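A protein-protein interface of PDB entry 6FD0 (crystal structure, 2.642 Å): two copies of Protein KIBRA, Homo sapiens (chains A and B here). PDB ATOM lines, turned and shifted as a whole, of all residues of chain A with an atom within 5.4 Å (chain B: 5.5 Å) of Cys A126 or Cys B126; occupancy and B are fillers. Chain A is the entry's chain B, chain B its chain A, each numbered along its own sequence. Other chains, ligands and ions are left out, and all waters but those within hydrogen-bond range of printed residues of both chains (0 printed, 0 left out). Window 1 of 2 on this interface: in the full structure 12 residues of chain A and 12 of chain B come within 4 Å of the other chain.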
ATOM      1  N   TYR A  23      12.733  20.157   9.371  1.00  0.00           N
ATOM      2  CA  TYR A  23      11.944  21.379   9.312  1.00  0.00           C
ATOM      3  C   TYR A  23      12.619  22.465  10.139  1.00  0.00           C
ATOM      4  O   TYR A  23      12.908  22.263  11.323  1.00  0.00           O
ATOM      5  CB  TYR A  23      10.520  21.139   9.805  1.00  0.00           C
ATOM      6  CG  TYR A  23       9.738  22.420   9.903  1.00  0.00           C
ATOM      7  CD1 TYR A  23       9.327  23.093   8.761  1.00  0.00           C
ATOM      8  CD2 TYR A  23       9.431  22.969  11.137  1.00  0.00           C
ATOM      9  CE1 TYR A  23       8.620  24.273   8.850  1.00  0.00           C
ATOM     10  CE2 TYR A  23       8.726  24.145  11.233  1.00  0.00           C
ATOM     11  CZ  TYR A  23       8.322  24.793  10.091  1.00  0.00           C
ATOM     12  OH  TYR A  23       7.619  25.970  10.196  1.00  0.00           O
ATOM     13  N   TYR A  91       4.706  25.281   9.883  1.00  0.00           N
ATOM     14  CA  TYR A  91       4.418  23.984  10.488  1.00  0.00           C
ATOM     15  C   TYR A  91       2.935  23.654  10.480  1.00  0.00           C
ATOM     16  O   TYR A  91       2.590  22.499  10.170  1.00  0.00           O
ATOM     17  CB  TYR A  91       4.966  23.924  11.920  1.00  0.00           C
ATOM     18  CG  TYR A  91       4.759  22.573  12.586  1.00  0.00           C
ATOM     19  CD1 TYR A  91       5.556  21.479  12.252  1.00  0.00           C
ATOM     20  CD2 TYR A  91       3.765  22.388  13.543  1.00  0.00           C
ATOM     21  CE1 TYR A  91       5.365  20.241  12.851  1.00  0.00           C
ATOM     22  CE2 TYR A  91       3.570  21.152  14.151  1.00  0.00           C
ATOM     23  CZ  TYR A  91       4.374  20.085  13.801  1.00  0.00           C
ATOM     24  OH  TYR A  91       4.187  18.855  14.399  1.00  0.00           O
ATOM     25  N   GLU A 124       4.953  12.953  11.406  1.00  0.00           N
ATOM     26  CA  GLU A 124       6.097  12.665  12.266  1.00  0.00           C
ATOM     27  C   GLU A 124       7.186  13.733  12.196  1.00  0.00           C
ATOM     28  O   GLU A 124       8.068  13.754  13.063  1.00  0.00           O
ATOM     29  CB  GLU A 124       6.719  11.310  11.897  1.00  0.00           C
ATOM     30  CG  GLU A 124       5.820  10.089  12.092  1.00  0.00           C
ATOM     31  CD  GLU A 124       6.565   8.766  11.876  1.00  0.00           C
ATOM     32  OE1 GLU A 124       7.751   8.673  12.262  1.00  0.00           O
ATOM     33  OE2 GLU A 124       5.971   7.818  11.315  1.00  0.00           O
ATOM     34  N   VAL A 125       7.156  14.611  11.190  1.00  0.00           N
ATOM     35  CA  VAL A 125       8.189  15.632  11.059  1.00  0.00           C
ATOM     36  C   VAL A 125       8.282  16.435  12.348  1.00  0.00           C
ATOM     37  O   VAL A 125       7.263  16.815  12.938  1.00  0.00           O
ATOM     38  CB  VAL A 125       7.906  16.536   9.847  1.00  0.00           C
ATOM     39  CG1 VAL A 125       8.992  17.598   9.693  1.00  0.00           C
ATOM     40  CG2 VAL A 125       7.813  15.699   8.585  1.00  0.00           C
ATOM     41  N   CYS A 126       9.509  16.664  12.808  1.00  0.00           N
ATOM     42  CA  CYS A 126       9.735  17.364  14.067  1.00  0.00           C
ATOM     43  C   CYS A 126       9.684  18.870  13.845  1.00  0.00           C
ATOM     44  O   CYS A 126      10.426  19.414  13.021  1.00  0.00           O
ATOM     45  CB  CYS A 126      11.088  16.991  14.679  1.00  0.00           C
ATOM     46  SG  CYS A 126      11.536  15.222  14.788  1.00  0.00           S
ATOM     47  N   ARG A 127       8.810  19.545  14.589  1.00  0.00           N
ATOM     48  CA  ARG A 127       8.790  21.005  14.587  1.00  0.00           C
ATOM     49  C   ARG A 127      10.086  21.564  15.163  1.00  0.00           C
ATOM     50  O   ARG A 127      10.588  22.595  14.693  1.00  0.00           O
ATOM     51  CB  ARG A 127       7.577  21.506  15.381  1.00  0.00           C
ATOM     52  CG  ARG A 127       7.405  23.020  15.422  1.00  0.00           C
ATOM     53  CD  ARG A 127       6.116  23.415  16.133  1.00  0.00           C
ATOM     54  NE  ARG A 127       6.115  22.991  17.532  1.00  0.00           N
ATOM     55  CZ  ARG A 127       6.658  23.683  18.532  1.00  0.00           C
ATOM     56  NH1 ARG A 127       7.253  24.847  18.303  1.00  0.00           N
ATOM     57  NH2 ARG A 127       6.607  23.212  19.771  1.00  0.00           N
ATOM     58  N   SER A 128      10.644  20.880  16.167  1.00  0.00           N
ATOM     59  CA  SER A 128      11.922  21.227  16.777  1.00  0.00           C
ATOM     60  C   SER A 128      13.104  21.099  15.825  1.00  0.00           C
ATOM     61  O   SER A 128      14.188  21.589  16.156  1.00  0.00           O
ATOM     62  CB  SER A 128      12.149  20.346  18.008  1.00  0.00           C
ATOM     63  OG  SER A 128      11.656  19.031  17.800  1.00  0.00           O
ATOM     64  N   GLY A 129      12.938  20.448  14.677  1.00  0.00           N
ATOM     65  CA  GLY A 129      13.956  20.424  13.645  1.00  0.00           C
ATOM     66  C   GLY A 129      14.714  19.120  13.510  1.00  0.00           C
ATOM     67  O   GLY A 129      15.479  18.981  12.553  1.00  0.00           O
ATOM     68  N   GLU A 130      14.534  18.154  14.409  1.00  0.00           N
ATOM     69  CA  GLU A 130      15.284  16.909  14.301  1.00  0.00           C
ATOM     70  C   GLU A 130      15.004  16.221  12.967  1.00  0.00           C
ATOM     71  O   GLU A 130      13.850  16.044  12.561  1.00  0.00           O
ATOM     72  CB  GLU A 130      14.949  15.969  15.461  1.00  0.00           C
ATOM     73  CG  GLU A 130      15.313  16.495  16.839  1.00  0.00           C
ATOM     74  CD  GLU A 130      14.213  17.345  17.448  1.00  0.00           C
ATOM     75  OE1 GLU A 130      13.328  17.794  16.695  1.00  0.00           O
ATOM     76  OE2 GLU A 130      14.222  17.557  18.679  1.00  0.00           O
ATOM     77  N   ARG A 131      16.078  15.826  12.294  1.00  0.00           N
ATOM     78  CA  ARG A 131      15.975  15.159  11.007  1.00  0.00           C
ATOM     79  C   ARG A 131      15.352  13.776  11.182  1.00  0.00           C
ATOM     80  O   ARG A 131      15.485  13.141  12.229  1.00  0.00           O
ATOM     81  CB  ARG A 131      17.366  15.056  10.372  1.00  0.00           C
ATOM     82  CG  ARG A 131      17.385  14.703   8.891  1.00  0.00           C
ATOM     83  CD  ARG A 131      18.808  14.685   8.317  1.00  0.00           C
ATOM     84  NE  ARG A 131      19.383  16.025   8.191  1.00  0.00           N
ATOM     85  CZ  ARG A 131      20.122  16.630   9.119  1.00  0.00           C
ATOM     86  NH1 ARG A 131      20.390  16.026  10.269  1.00  0.00           N
ATOM     87  NH2 ARG A 131      20.595  17.849   8.895  1.00  0.00           N
ATOM     88  N   LYS B  22       8.160   8.885  21.655  1.00  0.00           N
ATOM     89  CA  LYS B  22       7.565  10.200  21.844  1.00  0.00           C
ATOM     90  C   LYS B  22       8.164  10.820  23.094  1.00  0.00           C
ATOM     91  O   LYS B  22       8.225  10.161  24.135  1.00  0.00           O
ATOM     92  CB  LYS B  22       6.044  10.105  21.983  1.00  0.00           C
ATOM     93  CG  LYS B  22       5.335  11.450  22.034  1.00  0.00           C
ATOM     94  CD  LYS B  22       3.830  11.264  22.167  1.00  0.00           C
ATOM     95  CE  LYS B  22       3.094  12.587  22.177  1.00  0.00           C
ATOM     96  NZ  LYS B  22       1.687  12.417  22.662  1.00  0.00           N
ATOM     97  N   TYR B  23       8.588  12.076  22.999  1.00  0.00           N
ATOM     98  CA  TYR B  23       9.200  12.770  24.122  1.00  0.00           C
ATOM     99  C   TYR B  23       8.309  13.919  24.571  1.00  0.00           C
ATOM    100  O   TYR B  23       7.875  14.732  23.751  1.00  0.00           O
ATOM    101  CB  TYR B  23      10.588  13.289  23.758  1.00  0.00           C
ATOM    102  CG  TYR B  23      11.219  14.084  24.874  1.00  0.00           C
ATOM    103  CD1 TYR B  23      11.472  13.502  26.109  1.00  0.00           C
ATOM    104  CD2 TYR B  23      11.553  15.419  24.697  1.00  0.00           C
ATOM    105  CE1 TYR B  23      12.047  14.224  27.134  1.00  0.00           C
ATOM    106  CE2 TYR B  23      12.128  16.150  25.718  1.00  0.00           C
ATOM    107  CZ  TYR B  23      12.374  15.547  26.935  1.00  0.00           C
ATOM    108  OH  TYR B  23      12.946  16.264  27.963  1.00  0.00           O
ATOM    109  N   TYR B  91      15.828  16.390  27.283  1.00  0.00           N
ATOM    110  CA  TYR B  91      16.169  16.231  25.871  1.00  0.00           C
ATOM    111  C   TYR B  91      17.669  16.202  25.629  1.00  0.00           C
ATOM    112  O   TYR B  91      18.135  15.320  24.887  1.00  0.00           O
ATOM    113  CB  TYR B  91      15.506  17.334  25.036  1.00  0.00           C
ATOM    114  CG  TYR B  91      15.836  17.243  23.555  1.00  0.00           C
ATOM    115  CD1 TYR B  91      15.264  16.261  22.749  1.00  0.00           C
ATOM    116  CD2 TYR B  91      16.723  18.134  22.964  1.00  0.00           C
ATOM    117  CE1 TYR B  91      15.567  16.173  21.397  1.00  0.00           C
ATOM    118  CE2 TYR B  91      17.026  18.058  21.615  1.00  0.00           C
ATOM    119  CZ  TYR B  91      16.449  17.078  20.836  1.00  0.00           C
ATOM    120  OH  TYR B  91      16.759  17.009  19.495  1.00  0.00           O
ATOM    121  N   GLU B 124      17.038  11.377  16.380  1.00  0.00           N
ATOM    122  CA  GLU B 124      15.873  11.771  15.608  1.00  0.00           C
ATOM    123  C   GLU B 124      14.634  11.983  16.464  1.00  0.00           C
ATOM    124  O   GLU B 124      13.655  12.570  15.981  1.00  0.00           O
ATOM    125  CB  GLU B 124      15.578  10.718  14.536  1.00  0.00           C
ATOM    126  CG  GLU B 124      16.698  10.555  13.519  1.00  0.00           C
ATOM    127  CD  GLU B 124      16.190  10.070  12.187  1.00  0.00           C
ATOM    128  OE1 GLU B 124      15.187   9.329  12.172  1.00  0.00           O
ATOM    129  OE2 GLU B 124      16.788  10.447  11.158  1.00  0.00           O
ATOM    130  N   VAL B 125      14.641  11.514  17.714  1.00  0.00           N
ATOM    131  CA  VAL B 125      13.491  11.730  18.574  1.00  0.00           C
ATOM    132  C   VAL B 125      13.169  13.215  18.631  1.00  0.00           C
ATOM    133  O   VAL B 125      14.059  14.079  18.621  1.00  0.00           O
ATOM    134  CB  VAL B 125      13.706  11.155  19.982  1.00  0.00           C
ATOM    135  CG1 VAL B 125      12.477  11.387  20.857  1.00  0.00           C
ATOM    136  CG2 VAL B 125      13.995   9.691  19.875  1.00  0.00           C
ATOM    137  N   CYS B 126      11.873  13.529  18.576  1.00  0.00           N
ATOM    138  CA  CYS B 126      11.424  14.909  18.419  1.00  0.00           C
ATOM    139  C   CYS B 126      11.181  15.537  19.789  1.00  0.00           C
ATOM    140  O   CYS B 126      10.328  15.078  20.554  1.00  0.00           O
ATOM    141  CB  CYS B 126      10.152  15.029  17.574  1.00  0.00           C
ATOM    142  SG  CYS B 126      10.108  14.307  15.913  1.00  0.00           S
ATOM    143  N   ARG B 127      11.948  16.582  20.088  1.00  0.00           N
ATOM    144  CA  ARG B 127      11.723  17.392  21.286  1.00  0.00           C
ATOM    145  C   ARG B 127      10.316  17.983  21.288  1.00  0.00           C
ATOM    146  O   ARG B 127       9.689  18.107  22.347  1.00  0.00           O
ATOM    147  CB  ARG B 127      12.763  18.518  21.396  1.00  0.00           C
ATOM    148  CG  ARG B 127      12.722  19.232  22.745  1.00  0.00           C
ATOM    149  CD  ARG B 127      13.843  20.242  22.919  1.00  0.00           C
ATOM    150  NE  ARG B 127      13.927  20.681  24.311  1.00  0.00           N
ATOM    151  CZ  ARG B 127      15.015  21.183  24.890  1.00  0.00           C
ATOM    152  NH1 ARG B 127      16.145  21.322  24.210  1.00  0.00           N
ATOM    153  NH2 ARG B 127      14.970  21.544  26.164  1.00  0.00           N
ATOM    154  N   SER B 128       9.803  18.340  20.108  1.00  0.00           N
ATOM    155  CA  SER B 128       8.463  18.895  19.965  1.00  0.00           C
ATOM    156  C   SER B 128       7.363  17.919  20.366  1.00  0.00           C
ATOM    157  O   SER B 128       6.212  18.346  20.518  1.00  0.00           O
ATOM    158  CB  SER B 128       8.252  19.339  18.514  1.00  0.00           C
ATOM    159  OG  SER B 128       9.184  20.336  18.134  1.00  0.00           O
ATOM    160  N   GLY B 129       7.672  16.631  20.520  1.00  0.00           N
ATOM    161  CA  GLY B 129       6.716  15.655  21.012  1.00  0.00           C
ATOM    162  C   GLY B 129       5.984  14.835  19.968  1.00  0.00           C
ATOM    163  O   GLY B 129       5.045  14.116  20.326  1.00  0.00           O
ATOM    164  N   GLU B 130       6.368  14.906  18.697  1.00  0.00           N
ATOM    165  CA  GLU B 130       5.718  14.078  17.692  1.00  0.00           C
ATOM    166  C   GLU B 130       6.154  12.624  17.848  1.00  0.00           C
ATOM    167  O   GLU B 130       7.305  12.333  18.190  1.00  0.00           O
ATOM    168  CB  GLU B 130       6.045  14.555  16.276  1.00  0.00           C
ATOM    169  CG  GLU B 130       5.464  15.903  15.872  1.00  0.00           C
ATOM    170  CD  GLU B 130       6.297  17.073  16.345  1.00  0.00           C
ATOM    171  OE1 GLU B 130       6.925  16.955  17.414  1.00  0.00           O
ATOM    172  OE2 GLU B 130       6.329  18.106  15.640  1.00  0.00           O
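The side-chain hydroxyl (OH) of Tyr B91 lies within hydrogen-bond range of the side-chain carboxylate (OE2) of Glu A130 (2.7 Å). O of Val A125 lies close to OE2 of Glu B130 (3.1 Å). The side-chain carboxylate (OE2) of Glu B130 is in hydrogen-bond range of the backbone NH (N) of Arg A127 (3.1 Å). SG of Cys B126 forms a disulfide with SG of Cys A126. The side-chain hydroxyl of Tyr A91 sits at hydrogen-bond distance from the side-chain carboxylate of Glu B130, 2.6 Å away. The side-chain hydroxyl (OG) of Ser A128 is in hydrogen-bond range of the backbone NH (N) of Arg B127 (3.4 Å). The side-chain hydroxyl (OG) of Ser B128 is in hydrogen-bond range of the backbone NH (N) of Ser A128, at 2.5 Å. The backbone carbonyl oxygen (O) of Glu A124 sits close to the side-chain sulfur (SG) of Cys B126 (3.5 Å). The side-chain sulfur (SG) of Cys A126 lies close to the backbone carbonyl oxygen (O) of Glu B124, at 3.6 Å. N of Arg B127 is in hydrogen-bond range of OE2 of Glu A130, at 2.8 Å. O of Arg A131 lies close to OE2 of Glu B124 (3.2 Å). The side-chain carboxylate of Glu A130 sits close to the backbone carbonyl oxygen of Val B125 (3.5 Å).
Tyr A91 touches Glu B130, and with the chains exchanged Glu A130 touches Tyr B91. Glu A124 touches Cys B126, and with the chains exchanged Cys A126 touches Glu B124. Arg A127 touches Ser B128, and with the chains exchanged Ser A128 touches Arg B127. Ser B128 touches its own counterpart, Ser A128. 9 positions are printed for both chains. Of the 17 pairs that touch across the chains among the printed residues, 16 have their exchanged pair printed and touching as well.
Glu A124 touches Glu B130. Cys A126 touches Glu B130. Arg A127 touches Ser B128 (C to OG, 3.3 Å). Glu A130 touches Glu B124. Cys B126 touches Glu A130.
Tyr A23 touches none of the printed residues of chain B. Printed residues of chain B within 4 Å of Tyr A91: Glu B130 (2.6 Å). Printed residues of chain B within 4 Å of Cys A126: Glu B124 (3.6 Å), Cys B126 (2.0 Å) and Glu B130 (3.8 Å). Printed residues of chain A within 4 Å of Glu B124: Cys A126, Glu A130 and Arg A131. Printed residues of chain A within 4 Å of Val B125: Glu A130 (3.3 Å). The nearest printed residue of chain B that does not touch Ser A128 is Cys B126 (4.05 Å).
OE2 of Glu A130 sits close to OG of Ser A128 (3.1 Å). OH of Tyr A23 sits at hydrogen-bond distance from N of Tyr A91. OH of Tyr B23 sits at hydrogen-bond distance from N of Tyr B91, 3.0 Å away.
Printed residues of chain A that touch a printed residue of chain B: Tyr A91, Glu A124, Val A125, Cys A126, Arg A127, Ser A128, Glu A130 and Arg A131. Hydrophobic or aromatic side chains of chain A that line the printed part of chain B: Tyr A91. Printed residues of chain B that touch a printed residue of chain A: Tyr B91, Glu B124, Val B125, Cys B126, Arg B127, Ser B128 and Glu B130. Among the printed residues, 17 pairs touch across the chains. Among the printed residues, no Asp or Glu carboxylate lies within 4 Å of a Lys or Arg side-chain nitrogen of the other chain.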
